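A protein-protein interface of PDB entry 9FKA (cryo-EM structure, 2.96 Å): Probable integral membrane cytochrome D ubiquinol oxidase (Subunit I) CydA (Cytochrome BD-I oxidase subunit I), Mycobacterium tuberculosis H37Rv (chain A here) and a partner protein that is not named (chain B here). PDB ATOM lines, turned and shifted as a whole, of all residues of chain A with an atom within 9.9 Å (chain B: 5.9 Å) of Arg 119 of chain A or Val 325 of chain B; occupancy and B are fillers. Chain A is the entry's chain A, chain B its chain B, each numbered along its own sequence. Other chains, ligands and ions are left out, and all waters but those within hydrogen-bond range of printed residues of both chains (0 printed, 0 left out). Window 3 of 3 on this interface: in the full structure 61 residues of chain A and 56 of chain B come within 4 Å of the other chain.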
ATOM      1  N   THR A 108       5.545 -28.575  -9.064  1.00  0.00           N
ATOM      2  CA  THR A 108       5.562 -27.691 -10.224  1.00  0.00           C
ATOM      3  C   THR A 108       6.058 -26.301  -9.848  1.00  0.00           C
ATOM      4  O   THR A 108       6.881 -25.712 -10.558  1.00  0.00           O
ATOM      5  CB  THR A 108       4.168 -27.610 -10.845  1.00  0.00           C
ATOM      6  OG1 THR A 108       3.913 -28.793 -11.610  1.00  0.00           O
ATOM      7  CG2 THR A 108       4.053 -26.394 -11.753  1.00  0.00           C
ATOM      8  N   PHE A 109       5.567 -25.757  -8.734  1.00  0.00           N
ATOM      9  CA  PHE A 109       5.879 -24.380  -8.376  1.00  0.00           C
ATOM     10  C   PHE A 109       7.238 -24.230  -7.708  1.00  0.00           C
ATOM     11  O   PHE A 109       7.759 -23.111  -7.650  1.00  0.00           O
ATOM     12  CB  PHE A 109       4.792 -23.817  -7.463  1.00  0.00           C
ATOM     13  CG  PHE A 109       3.594 -23.304  -8.205  1.00  0.00           C
ATOM     14  CD1 PHE A 109       2.553 -24.151  -8.532  1.00  0.00           C
ATOM     15  CD2 PHE A 109       3.514 -21.977  -8.583  1.00  0.00           C
ATOM     16  CE1 PHE A 109       1.452 -23.682  -9.217  1.00  0.00           C
ATOM     17  CE2 PHE A 109       2.416 -21.504  -9.267  1.00  0.00           C
ATOM     18  CZ  PHE A 109       1.384 -22.356  -9.584  1.00  0.00           C
ATOM     19  N   GLY A 111       9.898 -25.634  -8.997  1.00  0.00           N
ATOM     20  CA  GLY A 111      10.729 -25.394 -10.164  1.00  0.00           C
ATOM     21  C   GLY A 111      10.663 -23.953 -10.631  1.00  0.00           C
ATOM     22  O   GLY A 111      11.681 -23.364 -11.003  1.00  0.00           O
ATOM     23  N   LEU A 112       9.466 -23.365 -10.618  1.00  0.00           N
ATOM     24  CA  LEU A 112       9.332 -21.964 -10.998  1.00  0.00           C
ATOM     25  C   LEU A 112      10.110 -21.063 -10.049  1.00  0.00           C
ATOM     26  O   LEU A 112      10.777 -20.117 -10.483  1.00  0.00           O
ATOM     27  CB  LEU A 112       7.859 -21.564 -11.020  1.00  0.00           C
ATOM     28  CG  LEU A 112       7.097 -21.889 -12.304  1.00  0.00           C
ATOM     29  CD1 LEU A 112       5.604 -21.929 -12.043  1.00  0.00           C
ATOM     30  CD2 LEU A 112       7.423 -20.872 -13.382  1.00  0.00           C
ATOM     31  N   TRP A 113      10.036 -21.341  -8.746  1.00  0.00           N
ATOM     32  CA  TRP A 113      10.735 -20.507  -7.777  1.00  0.00           C
ATOM     33  C   TRP A 113      12.240 -20.553  -7.996  1.00  0.00           C
ATOM     34  O   TRP A 113      12.917 -19.519  -7.937  1.00  0.00           O
ATOM     35  CB  TRP A 113      10.388 -20.955  -6.359  1.00  0.00           C
ATOM     36  CG  TRP A 113      10.961 -20.072  -5.300  1.00  0.00           C
ATOM     37  CD1 TRP A 113      10.594 -18.792  -5.015  1.00  0.00           C
ATOM     38  CD2 TRP A 113      12.006 -20.405  -4.381  1.00  0.00           C
ATOM     39  NE1 TRP A 113      11.346 -18.305  -3.974  1.00  0.00           N
ATOM     40  CE2 TRP A 113      12.221 -19.277  -3.567  1.00  0.00           C
ATOM     41  CE3 TRP A 113      12.781 -21.548  -4.166  1.00  0.00           C
ATOM     42  CZ2 TRP A 113      13.175 -19.258  -2.557  1.00  0.00           C
ATOM     43  CZ3 TRP A 113      13.728 -21.527  -3.163  1.00  0.00           C
ATOM     44  CH2 TRP A 113      13.918 -20.390  -2.371  1.00  0.00           C
ATOM     45  N   ILE A 114      12.786 -21.743  -8.250  1.00  0.00           N
ATOM     46  CA  ILE A 114      14.232 -21.883  -8.398  1.00  0.00           C
ATOM     47  C   ILE A 114      14.720 -21.104  -9.613  1.00  0.00           C
ATOM     48  O   ILE A 114      15.693 -20.344  -9.537  1.00  0.00           O
ATOM     49  CB  ILE A 114      14.617 -23.369  -8.498  1.00  0.00           C
ATOM     50  CG1 ILE A 114      14.279 -24.097  -7.199  1.00  0.00           C
ATOM     51  CG2 ILE A 114      16.095 -23.513  -8.803  1.00  0.00           C
ATOM     52  CD1 ILE A 114      14.099 -25.584  -7.373  1.00  0.00           C
ATOM     53  N   PHE A 115      14.050 -21.279 -10.751  1.00  0.00           N
ATOM     54  CA  PHE A 115      14.527 -20.731 -12.012  1.00  0.00           C
ATOM     55  C   PHE A 115      13.906 -19.389 -12.366  1.00  0.00           C
ATOM     56  O   PHE A 115      14.399 -18.719 -13.280  1.00  0.00           O
ATOM     57  CB  PHE A 115      14.245 -21.720 -13.146  1.00  0.00           C
ATOM     58  CG  PHE A 115      15.130 -22.929 -13.128  1.00  0.00           C
ATOM     59  CD1 PHE A 115      14.882 -23.968 -12.251  1.00  0.00           C
ATOM     60  CD2 PHE A 115      16.207 -23.029 -13.989  1.00  0.00           C
ATOM     61  CE1 PHE A 115      15.693 -25.082 -12.229  1.00  0.00           C
ATOM     62  CE2 PHE A 115      17.022 -24.142 -13.971  1.00  0.00           C
ATOM     63  CZ  PHE A 115      16.763 -25.169 -13.091  1.00  0.00           C
ATOM     64  N   GLY A 116      12.853 -18.977 -11.670  1.00  0.00           N
ATOM     65  CA  GLY A 116      12.140 -17.769 -12.032  1.00  0.00           C
ATOM     66  C   GLY A 116      12.621 -16.535 -11.298  1.00  0.00           C
ATOM     67  O   GLY A 116      11.907 -15.532 -11.232  1.00  0.00           O
ATOM     68  N   TRP A 117      13.830 -16.593 -10.739  1.00  0.00           N
ATOM     69  CA  TRP A 117      14.322 -15.478  -9.939  1.00  0.00           C
ATOM     70  C   TRP A 117      14.416 -14.204 -10.769  1.00  0.00           C
ATOM     71  O   TRP A 117      14.008 -13.126 -10.323  1.00  0.00           O
ATOM     72  CB  TRP A 117      15.680 -15.826  -9.332  1.00  0.00           C
ATOM     73  CG  TRP A 117      15.578 -16.338  -7.935  1.00  0.00           C
ATOM     74  CD1 TRP A 117      15.745 -17.624  -7.519  1.00  0.00           C
ATOM     75  CD2 TRP A 117      15.276 -15.573  -6.763  1.00  0.00           C
ATOM     76  NE1 TRP A 117      15.571 -17.709  -6.160  1.00  0.00           N
ATOM     77  CE2 TRP A 117      15.282 -16.462  -5.673  1.00  0.00           C
ATOM     78  CE3 TRP A 117      15.006 -14.222  -6.531  1.00  0.00           C
ATOM     79  CZ2 TRP A 117      15.026 -16.046  -4.371  1.00  0.00           C
ATOM     80  CZ3 TRP A 117      14.752 -13.811  -5.239  1.00  0.00           C
ATOM     81  CH2 TRP A 117      14.763 -14.718  -4.175  1.00  0.00           C
ATOM     82  N   ASN A 118      14.953 -14.307 -11.983  1.00  0.00           N
ATOM     83  CA  ASN A 118      15.125 -13.157 -12.858  1.00  0.00           C
ATOM     84  C   ASN A 118      14.156 -13.149 -14.030  1.00  0.00           C
ATOM     85  O   ASN A 118      14.199 -12.218 -14.842  1.00  0.00           O
ATOM     86  CB  ASN A 118      16.564 -13.110 -13.384  1.00  0.00           C
ATOM     87  CG  ASN A 118      17.238 -11.770 -13.137  1.00  0.00           C
ATOM     88  OD1 ASN A 118      16.649 -10.858 -12.557  1.00  0.00           O
ATOM     89  ND2 ASN A 118      18.483 -11.648 -13.580  1.00  0.00           N
ATOM     90  N   ARG A 119      13.287 -14.152 -14.146  1.00  0.00           N
ATOM     91  CA  ARG A 119      12.358 -14.252 -15.267  1.00  0.00           C
ATOM     92  C   ARG A 119      10.968 -13.744 -14.900  1.00  0.00           C
ATOM     93  O   ARG A 119      10.444 -12.834 -15.550  1.00  0.00           O
ATOM     94  CB  ARG A 119      12.287 -15.705 -15.751  1.00  0.00           C
ATOM     95  CG  ARG A 119      12.193 -15.847 -17.259  1.00  0.00           C
ATOM     96  CD  ARG A 119      12.181 -17.304 -17.681  1.00  0.00           C
ATOM     97  NE  ARG A 119      13.323 -18.039 -17.146  1.00  0.00           N
ATOM     98  CZ  ARG A 119      14.376 -18.432 -17.853  1.00  0.00           C
ATOM     99  NH1 ARG A 119      14.484 -18.171 -19.146  1.00  0.00           N
ATOM    100  NH2 ARG A 119      15.349 -19.105 -17.244  1.00  0.00           N
ATOM    101  N   LEU A 120      10.359 -14.316 -13.866  1.00  0.00           N
ATOM    102  CA  LEU A 120       9.030 -13.895 -13.466  1.00  0.00           C
ATOM    103  C   LEU A 120       9.092 -12.542 -12.760  1.00  0.00           C
ATOM    104  O   LEU A 120      10.113 -12.188 -12.168  1.00  0.00           O
ATOM    105  CB  LEU A 120       8.395 -14.923 -12.535  1.00  0.00           C
ATOM    106  CG  LEU A 120       8.613 -16.399 -12.864  1.00  0.00           C
ATOM    107  CD1 LEU A 120       8.088 -17.276 -11.743  1.00  0.00           C
ATOM    108  CD2 LEU A 120       7.937 -16.748 -14.172  1.00  0.00           C
ATOM    109  N   PRO A 121       8.013 -11.765 -12.806  1.00  0.00           N
ATOM    110  CA  PRO A 121       7.967 -10.536 -12.010  1.00  0.00           C
ATOM    111  C   PRO A 121       7.988 -10.853 -10.524  1.00  0.00           C
ATOM    112  O   PRO A 121       7.571 -11.928 -10.088  1.00  0.00           O
ATOM    113  CB  PRO A 121       6.645  -9.882 -12.429  1.00  0.00           C
ATOM    114  CG  PRO A 121       5.826 -10.984 -12.985  1.00  0.00           C
ATOM    115  CD  PRO A 121       6.783 -11.961 -13.590  1.00  0.00           C
ATOM    116  N   ARG A 122       8.494  -9.897  -9.742  1.00  0.00           N
ATOM    117  CA  ARG A 122       8.699 -10.134  -8.317  1.00  0.00           C
ATOM    118  C   ARG A 122       7.426 -10.640  -7.649  1.00  0.00           C
ATOM    119  O   ARG A 122       7.456 -11.609  -6.882  1.00  0.00           O
ATOM    120  CB  ARG A 122       9.184  -8.854  -7.639  1.00  0.00           C
ATOM    121  CG  ARG A 122      10.593  -8.445  -8.028  1.00  0.00           C
ATOM    122  CD  ARG A 122      11.205  -7.505  -7.004  1.00  0.00           C
ATOM    123  NE  ARG A 122      10.266  -6.483  -6.559  1.00  0.00           N
ATOM    124  CZ  ARG A 122      10.594  -5.443  -5.803  1.00  0.00           C
ATOM    125  NH1 ARG A 122      11.835  -5.254  -5.386  1.00  0.00           N
ATOM    126  NH2 ARG A 122       9.652  -4.571  -5.455  1.00  0.00           N
ATOM    127  N   LEU A 123       6.293  -9.997  -7.932  1.00  0.00           N
ATOM    128  CA  LEU A 123       5.048 -10.381  -7.276  1.00  0.00           C
ATOM    129  C   LEU A 123       4.681 -11.825  -7.596  1.00  0.00           C
ATOM    130  O   LEU A 123       4.345 -12.606  -6.700  1.00  0.00           O
ATOM    131  CB  LEU A 123       3.922  -9.436  -7.694  1.00  0.00           C
ATOM    132  CG  LEU A 123       3.874  -8.066  -7.012  1.00  0.00           C
ATOM    133  CD1 LEU A 123       3.778  -8.206  -5.501  1.00  0.00           C
ATOM    134  CD2 LEU A 123       5.084  -7.228  -7.395  1.00  0.00           C
ATOM    135  N   VAL A 124       4.743 -12.201  -8.875  1.00  0.00           N
ATOM    136  CA  VAL A 124       4.404 -13.569  -9.255  1.00  0.00           C
ATOM    137  C   VAL A 124       5.388 -14.550  -8.638  1.00  0.00           C
ATOM    138  O   VAL A 124       4.995 -15.592  -8.101  1.00  0.00           O
ATOM    139  CB  VAL A 124       4.358 -13.704 -10.787  1.00  0.00           C
ATOM    140  CG1 VAL A 124       4.283 -15.170 -11.186  1.00  0.00           C
ATOM    141  CG2 VAL A 124       3.175 -12.928 -11.346  1.00  0.00           C
ATOM    142  N   HIS A 125       6.683 -14.236  -8.702  1.00  0.00           N
ATOM    143  CA  HIS A 125       7.683 -15.127  -8.125  1.00  0.00           C
ATOM    144  C   HIS A 125       7.468 -15.289  -6.628  1.00  0.00           C
ATOM    145  O   HIS A 125       7.674 -16.376  -6.077  1.00  0.00           O
ATOM    146  CB  HIS A 125       9.085 -14.596  -8.415  1.00  0.00           C
ATOM    147  CG  HIS A 125      10.176 -15.551  -8.051  1.00  0.00           C
ATOM    148  ND1 HIS A 125      10.973 -15.382  -6.941  1.00  0.00           N
ATOM    149  CD2 HIS A 125      10.599 -16.691  -8.648  1.00  0.00           C
ATOM    150  CE1 HIS A 125      11.844 -16.373  -6.872  1.00  0.00           C
ATOM    151  NE2 HIS A 125      11.637 -17.181  -7.895  1.00  0.00           N
ATOM    152  N   LEU A 126       7.057 -14.216  -5.950  1.00  0.00           N
ATOM    153  CA  LEU A 126       6.751 -14.319  -4.529  1.00  0.00           C
ATOM    154  C   LEU A 126       5.606 -15.292  -4.287  1.00  0.00           C
ATOM    155  O   LEU A 126       5.635 -16.071  -3.328  1.00  0.00           O
ATOM    156  CB  LEU A 126       6.412 -12.938  -3.968  1.00  0.00           C
ATOM    157  CG  LEU A 126       5.815 -12.906  -2.562  1.00  0.00           C
ATOM    158  CD1 LEU A 126       6.759 -13.551  -1.566  1.00  0.00           C
ATOM    159  CD2 LEU A 126       5.502 -11.479  -2.157  1.00  0.00           C
ATOM    160  N   CYS A 128       4.938 -17.862  -5.964  1.00  0.00           N
ATOM    161  CA  CYS A 128       5.359 -19.234  -6.230  1.00  0.00           C
ATOM    162  C   CYS A 128       5.777 -19.939  -4.947  1.00  0.00           C
ATOM    163  O   CYS A 128       5.393 -21.088  -4.704  1.00  0.00           O
ATOM    164  CB  CYS A 128       6.501 -19.244  -7.245  1.00  0.00           C
ATOM    165  SG  CYS A 128       5.993 -18.876  -8.938  1.00  0.00           S
ATOM    166  N   THR B 320       1.225 -26.407 -18.347  1.00  0.00           N
ATOM    167  CA  THR B 320       1.587 -25.839 -19.641  1.00  0.00           C
ATOM    168  C   THR B 320       2.157 -24.440 -19.477  1.00  0.00           C
ATOM    169  O   THR B 320       3.066 -24.040 -20.212  1.00  0.00           O
ATOM    170  CB  THR B 320       0.372 -25.811 -20.567  1.00  0.00           C
ATOM    171  OG1 THR B 320      -0.626 -24.938 -20.025  1.00  0.00           O
ATOM    172  CG2 THR B 320      -0.209 -27.208 -20.744  1.00  0.00           C
ATOM    173  N   TRP B 321       1.628 -23.674 -18.521  1.00  0.00           N
ATOM    174  CA  TRP B 321       2.151 -22.335 -18.281  1.00  0.00           C
ATOM    175  C   TRP B 321       3.613 -22.386 -17.858  1.00  0.00           C
ATOM    176  O   TRP B 321       4.408 -21.523 -18.243  1.00  0.00           O
ATOM    177  CB  TRP B 321       1.313 -21.627 -17.221  1.00  0.00           C
ATOM    178  CG  TRP B 321       1.804 -20.255 -16.905  1.00  0.00           C
ATOM    179  CD1 TRP B 321       1.762 -19.162 -17.719  1.00  0.00           C
ATOM    180  CD2 TRP B 321       2.417 -19.823 -15.687  1.00  0.00           C
ATOM    181  NE1 TRP B 321       2.310 -18.076 -17.082  1.00  0.00           N
ATOM    182  CE2 TRP B 321       2.720 -18.457 -15.832  1.00  0.00           C
ATOM    183  CE3 TRP B 321       2.740 -20.461 -14.485  1.00  0.00           C
ATOM    184  CZ2 TRP B 321       3.328 -17.717 -14.825  1.00  0.00           C
ATOM    185  CZ3 TRP B 321       3.342 -19.724 -13.486  1.00  0.00           C
ATOM    186  CH2 TRP B 321       3.630 -18.367 -13.662  1.00  0.00           C
ATOM    187  N   THR B 322       3.984 -23.387 -17.059  1.00  0.00           N
ATOM    188  CA  THR B 322       5.379 -23.520 -16.653  1.00  0.00           C
ATOM    189  C   THR B 322       6.282 -23.709 -17.865  1.00  0.00           C
ATOM    190  O   THR B 322       7.347 -23.089 -17.958  1.00  0.00           O
ATOM    191  CB  THR B 322       5.536 -24.689 -15.684  1.00  0.00           C
ATOM    192  OG1 THR B 322       4.880 -24.381 -14.449  1.00  0.00           O
ATOM    193  CG2 THR B 322       7.004 -24.971 -15.416  1.00  0.00           C
ATOM    194  N   TYR B 323       5.872 -24.561 -18.804  1.00  0.00           N
ATOM    195  CA  TYR B 323       6.653 -24.748 -20.022  1.00  0.00           C
ATOM    196  C   TYR B 323       6.685 -23.473 -20.853  1.00  0.00           C
ATOM    197  O   TYR B 323       7.713 -23.139 -21.453  1.00  0.00           O
ATOM    198  CB  TYR B 323       6.078 -25.906 -20.833  1.00  0.00           C
ATOM    199  CG  TYR B 323       6.432 -27.262 -20.274  1.00  0.00           C
ATOM    200  CD1 TYR B 323       7.671 -27.831 -20.520  1.00  0.00           C
ATOM    201  CD2 TYR B 323       5.525 -27.975 -19.506  1.00  0.00           C
ATOM    202  CE1 TYR B 323       8.000 -29.070 -20.015  1.00  0.00           C
ATOM    203  CE2 TYR B 323       5.845 -29.214 -18.996  1.00  0.00           C
ATOM    204  CZ  TYR B 323       7.081 -29.758 -19.253  1.00  0.00           C
ATOM    205  OH  TYR B 323       7.404 -30.994 -18.745  1.00  0.00           O
ATOM    206  N   TRP B 324       5.567 -22.750 -20.904  1.00  0.00           N
ATOM    207  CA  TRP B 324       5.534 -21.498 -21.653  1.00  0.00           C
ATOM    208  C   TRP B 324       6.515 -20.489 -21.075  1.00  0.00           C
ATOM    209  O   TRP B 324       7.161 -19.742 -21.818  1.00  0.00           O
ATOM    210  CB  TRP B 324       4.120 -20.925 -21.654  1.00  0.00           C
ATOM    211  CG  TRP B 324       4.053 -19.520 -22.155  1.00  0.00           C
ATOM    212  CD1 TRP B 324       4.108 -18.382 -21.406  1.00  0.00           C
ATOM    213  CD2 TRP B 324       3.920 -19.099 -23.515  1.00  0.00           C
ATOM    214  NE1 TRP B 324       4.016 -17.278 -22.217  1.00  0.00           N
ATOM    215  CE2 TRP B 324       3.900 -17.692 -23.518  1.00  0.00           C
ATOM    216  CE3 TRP B 324       3.814 -19.777 -24.733  1.00  0.00           C
ATOM    217  CZ2 TRP B 324       3.779 -16.949 -24.688  1.00  0.00           C
ATOM    218  CZ3 TRP B 324       3.694 -19.038 -25.894  1.00  0.00           C
ATOM    219  CH2 TRP B 324       3.678 -17.639 -25.863  1.00  0.00           C
ATOM    220  N   VAL B 325       6.636 -20.447 -19.747  1.00  0.00           N
ATOM    221  CA  VAL B 325       7.533 -19.487 -19.112  1.00  0.00           C
ATOM    222  C   VAL B 325       8.968 -19.720 -19.563  1.00  0.00           C
ATOM    223  O   VAL B 325       9.692 -18.774 -19.892  1.00  0.00           O
ATOM    224  CB  VAL B 325       7.402 -19.573 -17.581  1.00  0.00           C
ATOM    225  CG1 VAL B 325       8.654 -19.040 -16.905  1.00  0.00           C
ATOM    226  CG2 VAL B 325       6.172 -18.817 -17.112  1.00  0.00           C
ATOM    227  N   PHE B 326       9.401 -20.980 -19.586  1.00  0.00           N
ATOM    228  CA  PHE B 326      10.764 -21.341 -19.956  1.00  0.00           C
ATOM    229  C   PHE B 326      10.874 -21.756 -21.418  1.00  0.00           C
ATOM    230  O   PHE B 326      11.726 -22.578 -21.768  1.00  0.00           O
ATOM    231  CB  PHE B 326      11.271 -22.460 -19.048  1.00  0.00           C
ATOM    232  CG  PHE B 326      11.158 -22.146 -17.587  1.00  0.00           C
ATOM    233  CD1 PHE B 326      11.811 -21.051 -17.051  1.00  0.00           C
ATOM    234  CD2 PHE B 326      10.396 -22.939 -16.751  1.00  0.00           C
ATOM    235  CE1 PHE B 326      11.708 -20.757 -15.709  1.00  0.00           C
ATOM    236  CE2 PHE B 326      10.290 -22.647 -15.409  1.00  0.00           C
ATOM    237  CZ  PHE B 326      10.947 -21.556 -14.888  1.00  0.00           C
ATOM    238  N   ARG B 327      10.024 -21.200 -22.282  1.00  0.00           N
ATOM    239  CA  ARG B 327      10.054 -21.572 -23.691  1.00  0.00           C
ATOM    240  C   ARG B 327      11.319 -21.097 -24.390  1.00  0.00           C
ATOM    241  O   ARG B 327      11.691 -21.669 -25.420  1.00  0.00           O
ATOM    242  CB  ARG B 327       8.828 -21.005 -24.407  1.00  0.00           C
ATOM    243  CG  ARG B 327       8.872 -19.503 -24.631  1.00  0.00           C
ATOM    244  CD  ARG B 327       7.566 -18.995 -25.209  1.00  0.00           C
ATOM    245  NE  ARG B 327       7.585 -17.552 -25.416  1.00  0.00           N
ATOM    246  CZ  ARG B 327       7.432 -16.655 -24.452  1.00  0.00           C
ATOM    247  NH1 ARG B 327       7.248 -17.015 -23.193  1.00  0.00           N
ATOM    248  NH2 ARG B 327       7.466 -15.362 -24.760  1.00  0.00           N
ATOM    249  N   GLN B 328      11.986 -20.075 -23.862  1.00  0.00           N
ATOM    250  CA  GLN B 328      13.167 -19.540 -24.525  1.00  0.00           C
ATOM    251  C   GLN B 328      14.260 -20.598 -24.603  1.00  0.00           C
ATOM    252  O   GLN B 328      14.523 -21.319 -23.638  1.00  0.00           O
ATOM    253  CB  GLN B 328      13.678 -18.308 -23.781  1.00  0.00           C
ATOM    254  CG  GLN B 328      14.308 -17.263 -24.685  1.00  0.00           C
ATOM    255  CD  GLN B 328      14.888 -16.097 -23.911  1.00  0.00           C
ATOM    256  OE1 GLN B 328      14.398 -15.744 -22.839  1.00  0.00           O
ATOM    257  NE2 GLN B 328      15.939 -15.492 -24.451  1.00  0.00           N
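CG2 of Thr 108 of chain A touches OG1 of Thr 322 of chain B (3.5 Å).
CD1 of Leu 112 of chain A touches CZ3 of Trp 321 of chain B (3.5 Å).
Leu 112 of chain A touches Thr 322 of chain B (CD1 to OG1, 3.5 Å).
Phe 326 of chain B touches Leu 112 of chain A.
Phe 115 of chain A touches Phe 326 of chain B.
Arg 119 of chain A touches Val 325 of chain B (CD to O, 3.6 Å).
Arg 119 of chain A touches Phe 326 of chain B (NE to CD1, 3.4 Å).
CD2 of Leu 120 of chain A touches CG1 of Val 325 of chain B (3.6 Å).
Printed residues of chain A that touch a printed residue of chain B: Thr 108, Leu 112, Phe 115, Arg 119 and Leu 120.
Hydrophobic or aromatic side chains of chain A that line the printed part of chain B: Leu 112, Phe 115 and Leu 120.
Of the 9 printed residues of chain B, 4 touch a printed residue of chain A.
Hydrophobic or aromatic side chains of chain B within 4 Å of the printed part of chain A: Trp 321, Val 325 and Phe 326.
Along chain B the printed residues that touch a printed residue of chain A span positions 321 to 326.
Among the printed residues, no Asp or Glu carboxylate lies within 4 Å of a Lys or Arg side-chain nitrogen of the other chain.
Of the printed residues of chain B, Thr 108 of chain A touches Thr 322 (3.5 Å).
Of the printed residues of chain B, Phe 115 of chain A touches Phe 326.
Of chain B, only Val 325 and Phe 326 come within 4 Å of Arg 119 of chain A.
Of the printed residues of chain B, Leu 120 of chain A touches Val 325.
Pro 121 of chain A touches none of the printed residues of chain B.
Of the printed residues of chain A, Trp 321 of chain B touches Leu 112 (3.5 Å).
Of the printed residues of chain A, Thr 322 of chain B touches Thr 108 (3.5 Å) and Leu 112 (3.5 Å).
Val 325 of chain B touches just these residues of chain A: Arg 119 and Leu 120.
Gln 328 of chain B touches none of the printed residues of chain A.
The nearest residue of chain B that does not touch Arg 119 of chain A is Gln 328 of chain B (4.4 Å).
The nearest residue of chain A that does not touch Val 325 of chain B is Leu 112 of chain A (4.2 Å).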
